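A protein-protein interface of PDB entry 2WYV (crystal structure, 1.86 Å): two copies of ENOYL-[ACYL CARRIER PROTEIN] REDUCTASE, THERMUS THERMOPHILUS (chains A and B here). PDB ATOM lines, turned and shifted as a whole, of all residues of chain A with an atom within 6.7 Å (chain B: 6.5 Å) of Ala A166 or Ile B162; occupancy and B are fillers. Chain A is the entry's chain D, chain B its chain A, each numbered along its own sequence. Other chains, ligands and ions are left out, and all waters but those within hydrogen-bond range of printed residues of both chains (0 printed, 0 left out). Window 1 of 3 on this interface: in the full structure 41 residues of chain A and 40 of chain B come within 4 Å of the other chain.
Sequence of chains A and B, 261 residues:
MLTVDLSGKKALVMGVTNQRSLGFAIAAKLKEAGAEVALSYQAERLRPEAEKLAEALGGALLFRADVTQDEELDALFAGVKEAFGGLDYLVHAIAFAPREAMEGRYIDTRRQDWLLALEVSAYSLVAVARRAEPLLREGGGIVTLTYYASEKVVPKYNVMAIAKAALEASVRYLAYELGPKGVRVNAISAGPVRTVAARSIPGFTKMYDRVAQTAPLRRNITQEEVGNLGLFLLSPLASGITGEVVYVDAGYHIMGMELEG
Printed residues of chain A that touch a printed residue of chain B: Leu A118, Ala A122, Tyr A123, Val A126, Ile A162, Ala A165, Ala A166, Ala A169, Ser A170 and Tyr A173.
Hydrophobic or aromatic side chains of chain A that line the printed part of chain B: Ala A122, Tyr A123, Val A126, Ile A162, Ala A165, Ala A166, Ala A169 and Tyr A173.
Hydrophobic or aromatic side chains of chain B within 4 Å of the printed part of chain A: Tyr B106, Trp B114, Ala B149, Ala B161, Ile B162, Ala B165 and Ala B166.
Among the printed residues, no Asp or Glu carboxylate lies within 4 Å of a Lys or Arg side-chain nitrogen of the other chain.
Among the printed residues, merely in contact across the chains: Tyr A173 with Ala B161, Val A126 with Tyr B106, Tyr A123 with Trp B114, Ser A170 with Ile B162, Ala A165 with Ala B165, Ala A166 with Ile B162, Leu A118 with Trp B114, Ile A162 with Ala B166, Tyr A173 with Tyr B106, Tyr A173 with Ile B162, Ala A122 with Trp B114, Ala A169 with Ile B162 and Ala A169 with Ala B165.
Ile A162 touches Ala B166, and with the chains exchanged Ala A166 touches Ile B162.
Ala A165 touches its own counterpart, Ala B165.
10 positions are printed for both chains.
Of the 15 pairs that touch across the chains among the printed residues, 3 have their exchanged pair printed and touching as well.
Ala A166 touches just one residue of chain B: Ile B162 (3.7 Å).
Of chain A, only Ala A166 (3.7 Å), Ala A169 (3.9 Å), Ser A170 (3.5 Å) and Tyr A173 (3.8 Å) come within 4 Å of Ile B162.
Of the printed residues of chain B, Ala A122 touches Trp B114.
Printed residues of chain A within 4 Å of Trp B114: Leu A118, Ala A122 and Tyr A123.
Lys B164 touches none of the printed residues of chain A.
Ala A163 touches none of the printed residues of chain B.
The nearest residue of chain B that does not touch Ala A166 is Ala B165 (4.7 Å).
The nearest printed residue of chain A that does not touch Ile B162 is Leu A167 (5.5 Å).
The side-chain hydroxyl (OH) of Tyr B106 lies within hydrogen-bond range of the side-chain hydroxyl (OG) of Ser A170 (2.9 Å).
O of Ala B149 sits at hydrogen-bond distance from OH of Tyr A173, at 3.2 Å.
OH of Tyr B106 sits at hydrogen-bond distance from NE1 of Trp B114 (3.0 Å).
O of Ala A166 is in hydrogen-bond range of OG of Ser A170, 2.7 Å away.
O of Leu A118 lies within hydrogen-bond range of N of Tyr A123, 3.1 Å away.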
ATOM      1  N   LEU A 118     -20.134  14.234 -11.036  1.00  0.00           N
ATOM      2  CA  LEU A 118     -19.228  15.293 -11.533  1.00  0.00           C
ATOM      3  C   LEU A 118     -19.984  16.577 -11.888  1.00  0.00           C
ATOM      4  O   LEU A 118     -19.512  17.720 -11.641  1.00  0.00           O
ATOM      5  CB  LEU A 118     -18.441  14.765 -12.733  1.00  0.00           C
ATOM      6  CG  LEU A 118     -17.079  14.108 -12.466  1.00  0.00           C
ATOM      7  CD1 LEU A 118     -16.062  15.192 -12.087  1.00  0.00           C
ATOM      8  CD2 LEU A 118     -17.149  13.031 -11.368  1.00  0.00           C
ATOM      9  N   SER A 121     -21.261  18.293  -8.399  1.00  0.00           N
ATOM     10  CA  SER A 121     -20.166  18.553  -7.440  1.00  0.00           C
ATOM     11  C   SER A 121     -18.956  19.330  -7.943  1.00  0.00           C
ATOM     12  O   SER A 121     -18.210  19.834  -7.089  1.00  0.00           O
ATOM     13  CB  SER A 121     -19.692  17.237  -6.822  1.00  0.00           C
ATOM     14  OG  SER A 121     -20.792  16.508  -6.316  1.00  0.00           O
ATOM     15  N   ALA A 122     -18.745  19.438  -9.279  1.00  0.00           N
ATOM     16  CA  ALA A 122     -17.612  20.207  -9.870  1.00  0.00           C
ATOM     17  C   ALA A 122     -18.038  21.206 -10.955  1.00  0.00           C
ATOM     18  O   ALA A 122     -17.705  22.411 -10.879  1.00  0.00           O
ATOM     19  CB  ALA A 122     -16.500  19.265 -10.456  1.00  0.00           C
ATOM     20  N   TYR A 123     -18.792  20.743 -11.947  1.00  0.00           N
ATOM     21  CA  TYR A 123     -19.189  21.687 -13.021  1.00  0.00           C
ATOM     22  C   TYR A 123     -20.017  22.838 -12.447  1.00  0.00           C
ATOM     23  O   TYR A 123     -19.955  23.956 -12.943  1.00  0.00           O
ATOM     24  CB  TYR A 123     -19.954  21.016 -14.151  1.00  0.00           C
ATOM     25  CG  TYR A 123     -20.415  22.039 -15.162  1.00  0.00           C
ATOM     26  CD1 TYR A 123     -19.496  22.635 -16.025  1.00  0.00           C
ATOM     27  CD2 TYR A 123     -21.714  22.506 -15.174  1.00  0.00           C
ATOM     28  CE1 TYR A 123     -19.891  23.617 -16.933  1.00  0.00           C
ATOM     29  CE2 TYR A 123     -22.117  23.503 -16.081  1.00  0.00           C
ATOM     30  CZ  TYR A 123     -21.179  24.046 -16.953  1.00  0.00           C
ATOM     31  OH  TYR A 123     -21.530  25.046 -17.851  1.00  0.00           O
ATOM     32  N   VAL A 126     -18.296  26.157 -12.033  1.00  0.00           N
ATOM     33  CA  VAL A 126     -18.010  26.953 -13.257  1.00  0.00           C
ATOM     34  C   VAL A 126     -19.303  27.691 -13.691  1.00  0.00           C
ATOM     35  O   VAL A 126     -19.279  28.878 -14.013  1.00  0.00           O
ATOM     36  CB  VAL A 126     -17.521  26.109 -14.418  1.00  0.00           C
ATOM     37  CG1 VAL A 126     -17.347  26.976 -15.683  1.00  0.00           C
ATOM     38  CG2 VAL A 126     -16.222  25.361 -14.037  1.00  0.00           C
ATOM     39  N   SER A 150      -9.567  13.843  -2.501  1.00  0.00           N
ATOM     40  CA  SER A 150      -9.001  14.280  -3.787  1.00  0.00           C
ATOM     41  C   SER A 150      -7.497  13.929  -3.970  1.00  0.00           C
ATOM     42  O   SER A 150      -7.023  13.696  -5.111  1.00  0.00           O
ATOM     43  CB  SER A 150      -9.191  15.779  -3.929  1.00  0.00           C
ATOM     44  OG  SER A 150      -8.476  16.435  -2.901  1.00  0.00           O
ATOM     45  N   ALA A 161     -14.381  11.564  -4.402  1.00  0.00           N
ATOM     46  CA  ALA A 161     -12.934  11.874  -4.382  1.00  0.00           C
ATOM     47  C   ALA A 161     -12.499  12.485  -5.731  1.00  0.00           C
ATOM     48  O   ALA A 161     -11.793  13.525  -5.788  1.00  0.00           O
ATOM     49  CB  ALA A 161     -12.134  10.598  -4.127  1.00  0.00           C
ATOM     50  N   ILE A 162     -12.952  11.851  -6.808  1.00  0.00           N
ATOM     51  CA  ILE A 162     -12.643  12.298  -8.194  1.00  0.00           C
ATOM     52  C   ILE A 162     -13.343  13.641  -8.509  1.00  0.00           C
ATOM     53  O   ILE A 162     -12.745  14.520  -9.173  1.00  0.00           O
ATOM     54  CB  ILE A 162     -12.990  11.192  -9.242  1.00  0.00           C
ATOM     55  CG1 ILE A 162     -11.943  10.051  -9.254  1.00  0.00           C
ATOM     56  CG2 ILE A 162     -13.047  11.789 -10.657  1.00  0.00           C
ATOM     57  CD1 ILE A 162     -11.817   9.200  -7.997  1.00  0.00           C
ATOM     58  N   ALA A 163     -14.588  13.844  -8.046  1.00  0.00           N
ATOM     59  CA  ALA A 163     -15.256  15.160  -8.252  1.00  0.00           C
ATOM     60  C   ALA A 163     -14.517  16.306  -7.527  1.00  0.00           C
ATOM     61  O   ALA A 163     -14.387  17.443  -8.060  1.00  0.00           O
ATOM     62  CB  ALA A 163     -16.702  15.112  -7.794  1.00  0.00           C
ATOM     63  N   LYS A 164     -14.041  16.027  -6.309  1.00  0.00           N
ATOM     64  CA  LYS A 164     -13.254  17.023  -5.545  1.00  0.00           C
ATOM     65  C   LYS A 164     -11.915  17.362  -6.221  1.00  0.00           C
ATOM     66  O   LYS A 164     -11.443  18.499  -6.135  1.00  0.00           O
ATOM     67  CB  LYS A 164     -13.035  16.580  -4.078  1.00  0.00           C
ATOM     68  CG  LYS A 164     -14.354  16.464  -3.229  1.00  0.00           C
ATOM     69  CD  LYS A 164     -15.230  17.734  -3.258  1.00  0.00           C
ATOM     70  CE  LYS A 164     -16.342  17.730  -2.184  1.00  0.00           C
ATOM     71  NZ  LYS A 164     -17.230  18.920  -2.324  1.00  0.00           N
ATOM     72  N   ALA A 165     -11.273  16.405  -6.882  1.00  0.00           N
ATOM     73  CA  ALA A 165     -10.064  16.722  -7.659  1.00  0.00           C
ATOM     74  C   ALA A 165     -10.390  17.674  -8.791  1.00  0.00           C
ATOM     75  O   ALA A 165      -9.652  18.650  -9.054  1.00  0.00           O
ATOM     76  CB  ALA A 165      -9.412  15.431  -8.243  1.00  0.00           C
ATOM     77  N   ALA A 166     -11.489  17.411  -9.478  1.00  0.00           N
ATOM     78  CA  ALA A 166     -11.952  18.323 -10.577  1.00  0.00           C
ATOM     79  C   ALA A 166     -12.314  19.716 -10.074  1.00  0.00           C
ATOM     80  O   ALA A 166     -12.068  20.726 -10.777  1.00  0.00           O
ATOM     81  CB  ALA A 166     -13.167  17.727 -11.319  1.00  0.00           C
ATOM     82  N   LEU A 167     -12.912  19.802  -8.885  1.00  0.00           N
ATOM     83  CA  LEU A 167     -13.290  21.124  -8.306  1.00  0.00           C
ATOM     84  C   LEU A 167     -12.062  21.976  -7.947  1.00  0.00           C
ATOM     85  O   LEU A 167     -12.037  23.193  -8.196  1.00  0.00           O
ATOM     86  CB  LEU A 167     -14.152  20.915  -7.063  1.00  0.00           C
ATOM     87  CG  LEU A 167     -14.774  22.016  -6.195  1.00  0.00           C
ATOM     88  CD1 LEU A 167     -15.915  22.694  -6.903  1.00  0.00           C
ATOM     89  CD2 LEU A 167     -15.291  21.421  -4.832  1.00  0.00           C
ATOM     90  N   GLU A 168     -11.073  21.355  -7.314  1.00  0.00           N
ATOM     91  CA  GLU A 168      -9.863  22.060  -6.896  1.00  0.00           C
ATOM     92  C   GLU A 168      -9.106  22.586  -8.110  1.00  0.00           C
ATOM     93  O   GLU A 168      -8.676  23.742  -8.103  1.00  0.00           O
ATOM     94  CB  GLU A 168      -8.976  21.170  -6.017  1.00  0.00           C
ATOM     95  CG  GLU A 168      -9.606  20.859  -4.616  1.00  0.00           C
ATOM     96  CD  GLU A 168      -8.787  19.897  -3.762  1.00  0.00           C
ATOM     97  OE1 GLU A 168      -9.366  19.302  -2.811  1.00  0.00           O
ATOM     98  OE2 GLU A 168      -7.572  19.694  -4.044  1.00  0.00           O
ATOM     99  N   ALA A 169      -8.978  21.776  -9.149  1.00  0.00           N
ATOM    100  CA  ALA A 169      -8.410  22.271 -10.453  1.00  0.00           C
ATOM    101  C   ALA A 169      -9.216  23.445 -11.052  1.00  0.00           C
ATOM    102  O   ALA A 169      -8.619  24.398 -11.595  1.00  0.00           O
ATOM    103  CB  ALA A 169      -8.306  21.134 -11.461  1.00  0.00           C
ATOM    104  N   SER A 170     -10.551  23.406 -10.931  1.00  0.00           N
ATOM    105  CA  SER A 170     -11.387  24.518 -11.423  1.00  0.00           C
ATOM    106  C   SER A 170     -11.170  25.783 -10.593  1.00  0.00           C
ATOM    107  O   SER A 170     -11.099  26.904 -11.149  1.00  0.00           O
ATOM    108  CB  SER A 170     -12.881  24.176 -11.482  1.00  0.00           C
ATOM    109  OG  SER A 170     -13.171  22.878 -12.029  1.00  0.00           O
ATOM    110  N   VAL A 171     -11.018  25.644  -9.274  1.00  0.00           N
ATOM    111  CA  VAL A 171     -10.637  26.796  -8.406  1.00  0.00           C
ATOM    112  C   VAL A 171      -9.403  27.555  -8.928  1.00  0.00           C
ATOM    113  O   VAL A 171      -9.368  28.811  -8.945  1.00  0.00           O
ATOM    114  CB  VAL A 171     -10.385  26.357  -6.924  1.00  0.00           C
ATOM    115  CG1 VAL A 171      -9.613  27.452  -6.106  1.00  0.00           C
ATOM    116  CG2 VAL A 171     -11.711  26.033  -6.251  1.00  0.00           C
ATOM    117  N   TYR A 173      -8.027  27.527 -12.110  1.00  0.00           N
ATOM    118  CA  TYR A 173      -8.268  28.177 -13.442  1.00  0.00           C
ATOM    119  C   TYR A 173      -9.188  29.378 -13.306  1.00  0.00           C
ATOM    120  O   TYR A 173      -8.979  30.404 -13.972  1.00  0.00           O
ATOM    121  CB  TYR A 173      -8.734  27.159 -14.524  1.00  0.00           C
ATOM    122  CG  TYR A 173      -7.540  26.376 -15.109  1.00  0.00           C
ATOM    123  CD1 TYR A 173      -6.930  26.757 -16.305  1.00  0.00           C
ATOM    124  CD2 TYR A 173      -6.999  25.271 -14.429  1.00  0.00           C
ATOM    125  CE1 TYR A 173      -5.822  26.064 -16.815  1.00  0.00           C
ATOM    126  CE2 TYR A 173      -5.893  24.563 -14.928  1.00  0.00           C
ATOM    127  CZ  TYR A 173      -5.299  24.982 -16.120  1.00  0.00           C
ATOM    128  OH  TYR A 173      -4.210  24.292 -16.611  1.00  0.00           O
ATOM    129  N   TYR B 106     -11.884  29.190 -19.796  1.00  0.00           N
ATOM    130  CA  TYR B 106     -12.435  28.076 -18.994  1.00  0.00           C
ATOM    131  C   TYR B 106     -13.772  28.431 -18.338  1.00  0.00           C
ATOM    132  O   TYR B 106     -14.698  27.588 -18.270  1.00  0.00           O
ATOM    133  CB  TYR B 106     -11.461  27.642 -17.877  1.00  0.00           C
ATOM    134  CG  TYR B 106     -12.025  26.490 -17.063  1.00  0.00           C
ATOM    135  CD1 TYR B 106     -12.326  25.270 -17.686  1.00  0.00           C
ATOM    136  CD2 TYR B 106     -12.280  26.632 -15.706  1.00  0.00           C
ATOM    137  CE1 TYR B 106     -12.884  24.166 -16.932  1.00  0.00           C
ATOM    138  CE2 TYR B 106     -12.842  25.540 -14.940  1.00  0.00           C
ATOM    139  CZ  TYR B 106     -13.150  24.345 -15.579  1.00  0.00           C
ATOM    140  OH  TYR B 106     -13.685  23.297 -14.857  1.00  0.00           O
ATOM    141  N   TRP B 114     -18.397  20.235 -21.363  1.00  0.00           N
ATOM    142  CA  TRP B 114     -17.596  19.932 -20.174  1.00  0.00           C
ATOM    143  C   TRP B 114     -17.791  18.473 -19.795  1.00  0.00           C
ATOM    144  O   TRP B 114     -16.825  17.727 -19.575  1.00  0.00           O
ATOM    145  CB  TRP B 114     -18.014  20.843 -19.030  1.00  0.00           C
ATOM    146  CG  TRP B 114     -17.163  20.816 -17.741  1.00  0.00           C
ATOM    147  CD1 TRP B 114     -16.194  21.740 -17.373  1.00  0.00           C
ATOM    148  CD2 TRP B 114     -17.289  19.910 -16.614  1.00  0.00           C
ATOM    149  NE1 TRP B 114     -15.715  21.450 -16.133  1.00  0.00           N
ATOM    150  CE2 TRP B 114     -16.353  20.329 -15.642  1.00  0.00           C
ATOM    151  CE3 TRP B 114     -18.067  18.770 -16.355  1.00  0.00           C
ATOM    152  CZ2 TRP B 114     -16.194  19.670 -14.428  1.00  0.00           C
ATOM    153  CZ3 TRP B 114     -17.902  18.112 -15.145  1.00  0.00           C
ATOM    154  CH2 TRP B 114     -16.970  18.547 -14.204  1.00  0.00           C
ATOM    155  N   LEU B 118     -15.004  15.313 -19.886  1.00  0.00           N
ATOM    156  CA  LEU B 118     -14.820  14.454 -18.718  1.00  0.00           C
ATOM    157  C   LEU B 118     -15.165  12.979 -18.989  1.00  0.00           C
ATOM    158  O   LEU B 118     -14.414  12.098 -18.573  1.00  0.00           O
ATOM    159  CB  LEU B 118     -15.588  14.981 -17.516  1.00  0.00           C
ATOM    160  CG  LEU B 118     -14.883  15.945 -16.548  1.00  0.00           C
ATOM    161  CD1 LEU B 118     -13.875  15.201 -15.640  1.00  0.00           C
ATOM    162  CD2 LEU B 118     -14.203  17.091 -17.352  1.00  0.00           C
ATOM    163  N   ALA B 122     -11.670  10.836 -18.872  1.00  0.00           N
ATOM    164  CA  ALA B 122     -11.496  10.378 -17.471  1.00  0.00           C
ATOM    165  C   ALA B 122     -12.366   9.170 -17.179  1.00  0.00           C
ATOM    166  O   ALA B 122     -11.836   8.151 -16.821  1.00  0.00           O
ATOM    167  CB  ALA B 122     -11.813  11.512 -16.468  1.00  0.00           C
ATOM    168  N   ALA B 149      -0.648  20.656 -16.396  1.00  0.00           N
ATOM    169  CA  ALA B 149      -1.843  21.507 -16.322  1.00  0.00           C
ATOM    170  C   ALA B 149      -2.871  21.014 -15.274  1.00  0.00           C
ATOM    171  O   ALA B 149      -3.651  21.809 -14.747  1.00  0.00           O
ATOM    172  CB  ALA B 149      -2.501  21.633 -17.715  1.00  0.00           C
ATOM    173  N   SER B 150      -2.872  19.716 -14.979  1.00  0.00           N
ATOM    174  CA  SER B 150      -3.678  19.188 -13.851  1.00  0.00           C
ATOM    175  C   SER B 150      -3.383  19.899 -12.509  1.00  0.00           C
ATOM    176  O   SER B 150      -4.297  20.217 -11.761  1.00  0.00           O
ATOM    177  CB  SER B 150      -3.472  17.676 -13.717  1.00  0.00           C
ATOM    178  OG  SER B 150      -2.151  17.380 -13.289  1.00  0.00           O
ATOM    179  N   TYR B 157      -5.369  25.613 -21.530  1.00  0.00           N
ATOM    180  CA  TYR B 157      -5.550  24.147 -21.471  1.00  0.00           C
ATOM    181  C   TYR B 157      -6.980  23.809 -21.024  1.00  0.00           C
ATOM    182  O   TYR B 157      -7.487  22.730 -21.314  1.00  0.00           O
ATOM    183  CB  TYR B 157      -4.513  23.464 -20.546  1.00  0.00           C
ATOM    184  CG  TYR B 157      -3.262  22.997 -21.232  1.00  0.00           C
ATOM    185  CD1 TYR B 157      -3.027  21.637 -21.482  1.00  0.00           C
ATOM    186  CD2 TYR B 157      -2.297  23.915 -21.649  1.00  0.00           C
ATOM    187  CE1 TYR B 157      -1.853  21.220 -22.123  1.00  0.00           C
ATOM    188  CE2 TYR B 157      -1.136  23.510 -22.281  1.00  0.00           C
ATOM    189  CZ  TYR B 157      -0.907  22.177 -22.520  1.00  0.00           C
ATOM    190  OH  TYR B 157       0.275  21.840 -23.167  1.00  0.00           O
ATOM    191  N   ASN B 158      -7.601  24.738 -20.300  1.00  0.00           N
ATOM    192  CA  ASN B 158      -9.037  24.744 -20.006  1.00  0.00           C
ATOM    193  C   ASN B 158      -9.576  23.405 -19.428  1.00  0.00           C
ATOM    194  O   ASN B 158      -8.955  22.843 -18.517  1.00  0.00           O
ATOM    195  CB  ASN B 158      -9.773  25.210 -21.264  1.00  0.00           C
ATOM    196  CG  ASN B 158      -9.596  26.696 -21.523  1.00  0.00           C
ATOM    197  OD1 ASN B 158      -8.860  27.377 -20.824  1.00  0.00           O
ATOM    198  ND2 ASN B 158     -10.281  27.199 -22.532  1.00  0.00           N
ATOM    199  N   VAL B 159     -10.654  22.847 -19.983  1.00  0.00           N
ATOM    200  CA  VAL B 159     -11.262  21.625 -19.386  1.00  0.00           C
ATOM    201  C   VAL B 159     -10.381  20.358 -19.433  1.00  0.00           C
ATOM    202  O   VAL B 159     -10.590  19.382 -18.657  1.00  0.00           O
ATOM    203  CB  VAL B 159     -12.652  21.323 -20.028  1.00  0.00           C
ATOM    204  CG1 VAL B 159     -12.528  20.935 -21.518  1.00  0.00           C
ATOM    205  CG2 VAL B 159     -13.416  20.238 -19.235  1.00  0.00           C
ATOM    206  N   MET B 160      -9.412  20.319 -20.333  1.00  0.00           N
ATOM    207  CA  MET B 160      -8.472  19.185 -20.362  1.00  0.00           C
ATOM    208  C   MET B 160      -7.609  19.104 -19.086  1.00  0.00           C
ATOM    209  O   MET B 160      -7.323  18.003 -18.627  1.00  0.00           O
ATOM    210  CB  MET B 160      -7.573  19.228 -21.606  1.00  0.00           C
ATOM    211  CG  MET B 160      -8.253  18.774 -22.880  1.00  0.00           C
ATOM    212  SD  MET B 160      -9.034  17.140 -22.861  1.00  0.00           S
ATOM    213  CE  MET B 160      -7.703  16.118 -22.223  1.00  0.00           C
ATOM    214  N   ALA B 161      -7.219  20.259 -18.528  1.00  0.00           N
ATOM    215  CA  ALA B 161      -6.531  20.329 -17.243  1.00  0.00           C
ATOM    216  C   ALA B 161      -7.397  19.723 -16.143  1.00  0.00           C
ATOM    217  O   ALA B 161      -6.901  18.948 -15.301  1.00  0.00           O
ATOM    218  CB  ALA B 161      -6.150  21.756 -16.886  1.00  0.00           C
ATOM    219  N   ILE B 162      -8.699  20.029 -16.177  1.00  0.00           N
ATOM    220  CA  ILE B 162      -9.639  19.486 -15.174  1.00  0.00           C
ATOM    221  C   ILE B 162      -9.869  17.973 -15.382  1.00  0.00           C
ATOM    222  O   ILE B 162      -9.910  17.197 -14.405  1.00  0.00           O
ATOM    223  CB  ILE B 162     -11.001  20.311 -15.119  1.00  0.00           C
ATOM    224  CG1 ILE B 162     -10.823  21.633 -14.368  1.00  0.00           C
ATOM    225  CG2 ILE B 162     -12.101  19.526 -14.360  1.00  0.00           C
ATOM    226  CD1 ILE B 162      -9.719  22.590 -14.834  1.00  0.00           C
ATOM    227  N   ALA B 163      -9.994  17.527 -16.627  1.00  0.00           N
ATOM    228  CA  ALA B 163     -10.144  16.090 -16.915  1.00  0.00           C
ATOM    229  C   ALA B 163      -8.910  15.303 -16.426  1.00  0.00           C
ATOM    230  O   ALA B 163      -9.039  14.193 -15.879  1.00  0.00           O
ATOM    231  CB  ALA B 163     -10.367  15.833 -18.418  1.00  0.00           C
ATOM    232  N   LYS B 164      -7.722  15.858 -16.616  1.00  0.00           N
ATOM    233  CA  LYS B 164      -6.478  15.187 -16.168  1.00  0.00           C
ATOM    234  C   LYS B 164      -6.387  15.082 -14.635  1.00  0.00           C
ATOM    235  O   LYS B 164      -5.914  14.077 -14.129  1.00  0.00           O
ATOM    236  CB  LYS B 164      -5.240  15.876 -16.749  1.00  0.00           C
ATOM    237  CG  LYS B 164      -5.068  15.722 -18.247  1.00  0.00           C
ATOM    238  CD  LYS B 164      -5.236  14.293 -18.783  1.00  0.00           C
ATOM    239  CE  LYS B 164      -4.750  14.167 -20.260  1.00  0.00           C
ATOM    240  NZ  LYS B 164      -4.739  12.775 -20.761  1.00  0.00           N
ATOM    241  N   ALA B 165      -6.894  16.073 -13.902  1.00  0.00           N
ATOM    242  CA  ALA B 165      -6.955  15.987 -12.432  1.00  0.00           C
ATOM    243  C   ALA B 165      -7.866  14.844 -11.973  1.00  0.00           C
ATOM    244  O   ALA B 165      -7.529  14.098 -11.032  1.00  0.00           O
ATOM    245  CB  ALA B 165      -7.419  17.329 -11.828  1.00  0.00           C
ATOM    246  N   ALA B 166      -9.017  14.725 -12.630  1.00  0.00           N
ATOM    247  CA  ALA B 166      -9.962  13.605 -12.414  1.00  0.00           C
ATOM    248  C   ALA B 166      -9.359  12.239 -12.710  1.00  0.00           C
ATOM    249  O   ALA B 166      -9.613  11.244 -11.990  1.00  0.00           O
ATOM    250  CB  ALA B 166     -11.213  13.802 -13.287  1.00  0.00           C
ATOM    251  N   LEU B 167      -8.594  12.175 -13.791  1.00  0.00           N
ATOM    252  CA  LEU B 167      -7.903  10.962 -14.220  1.00  0.00           C
ATOM    253  C   LEU B 167      -6.837  10.527 -13.216  1.00  0.00           C
ATOM    254  O   LEU B 167      -6.757   9.319 -12.864  1.00  0.00           O
ATOM    255  CB  LEU B 167      -7.295  11.207 -15.630  1.00  0.00           C
ATOM    256  CG  LEU B 167      -6.579  10.057 -16.319  1.00  0.00           C
ATOM    257  CD1 LEU B 167      -7.617   8.966 -16.678  1.00  0.00           C
ATOM    258  CD2 LEU B 167      -5.882  10.534 -17.601  1.00  0.00           C
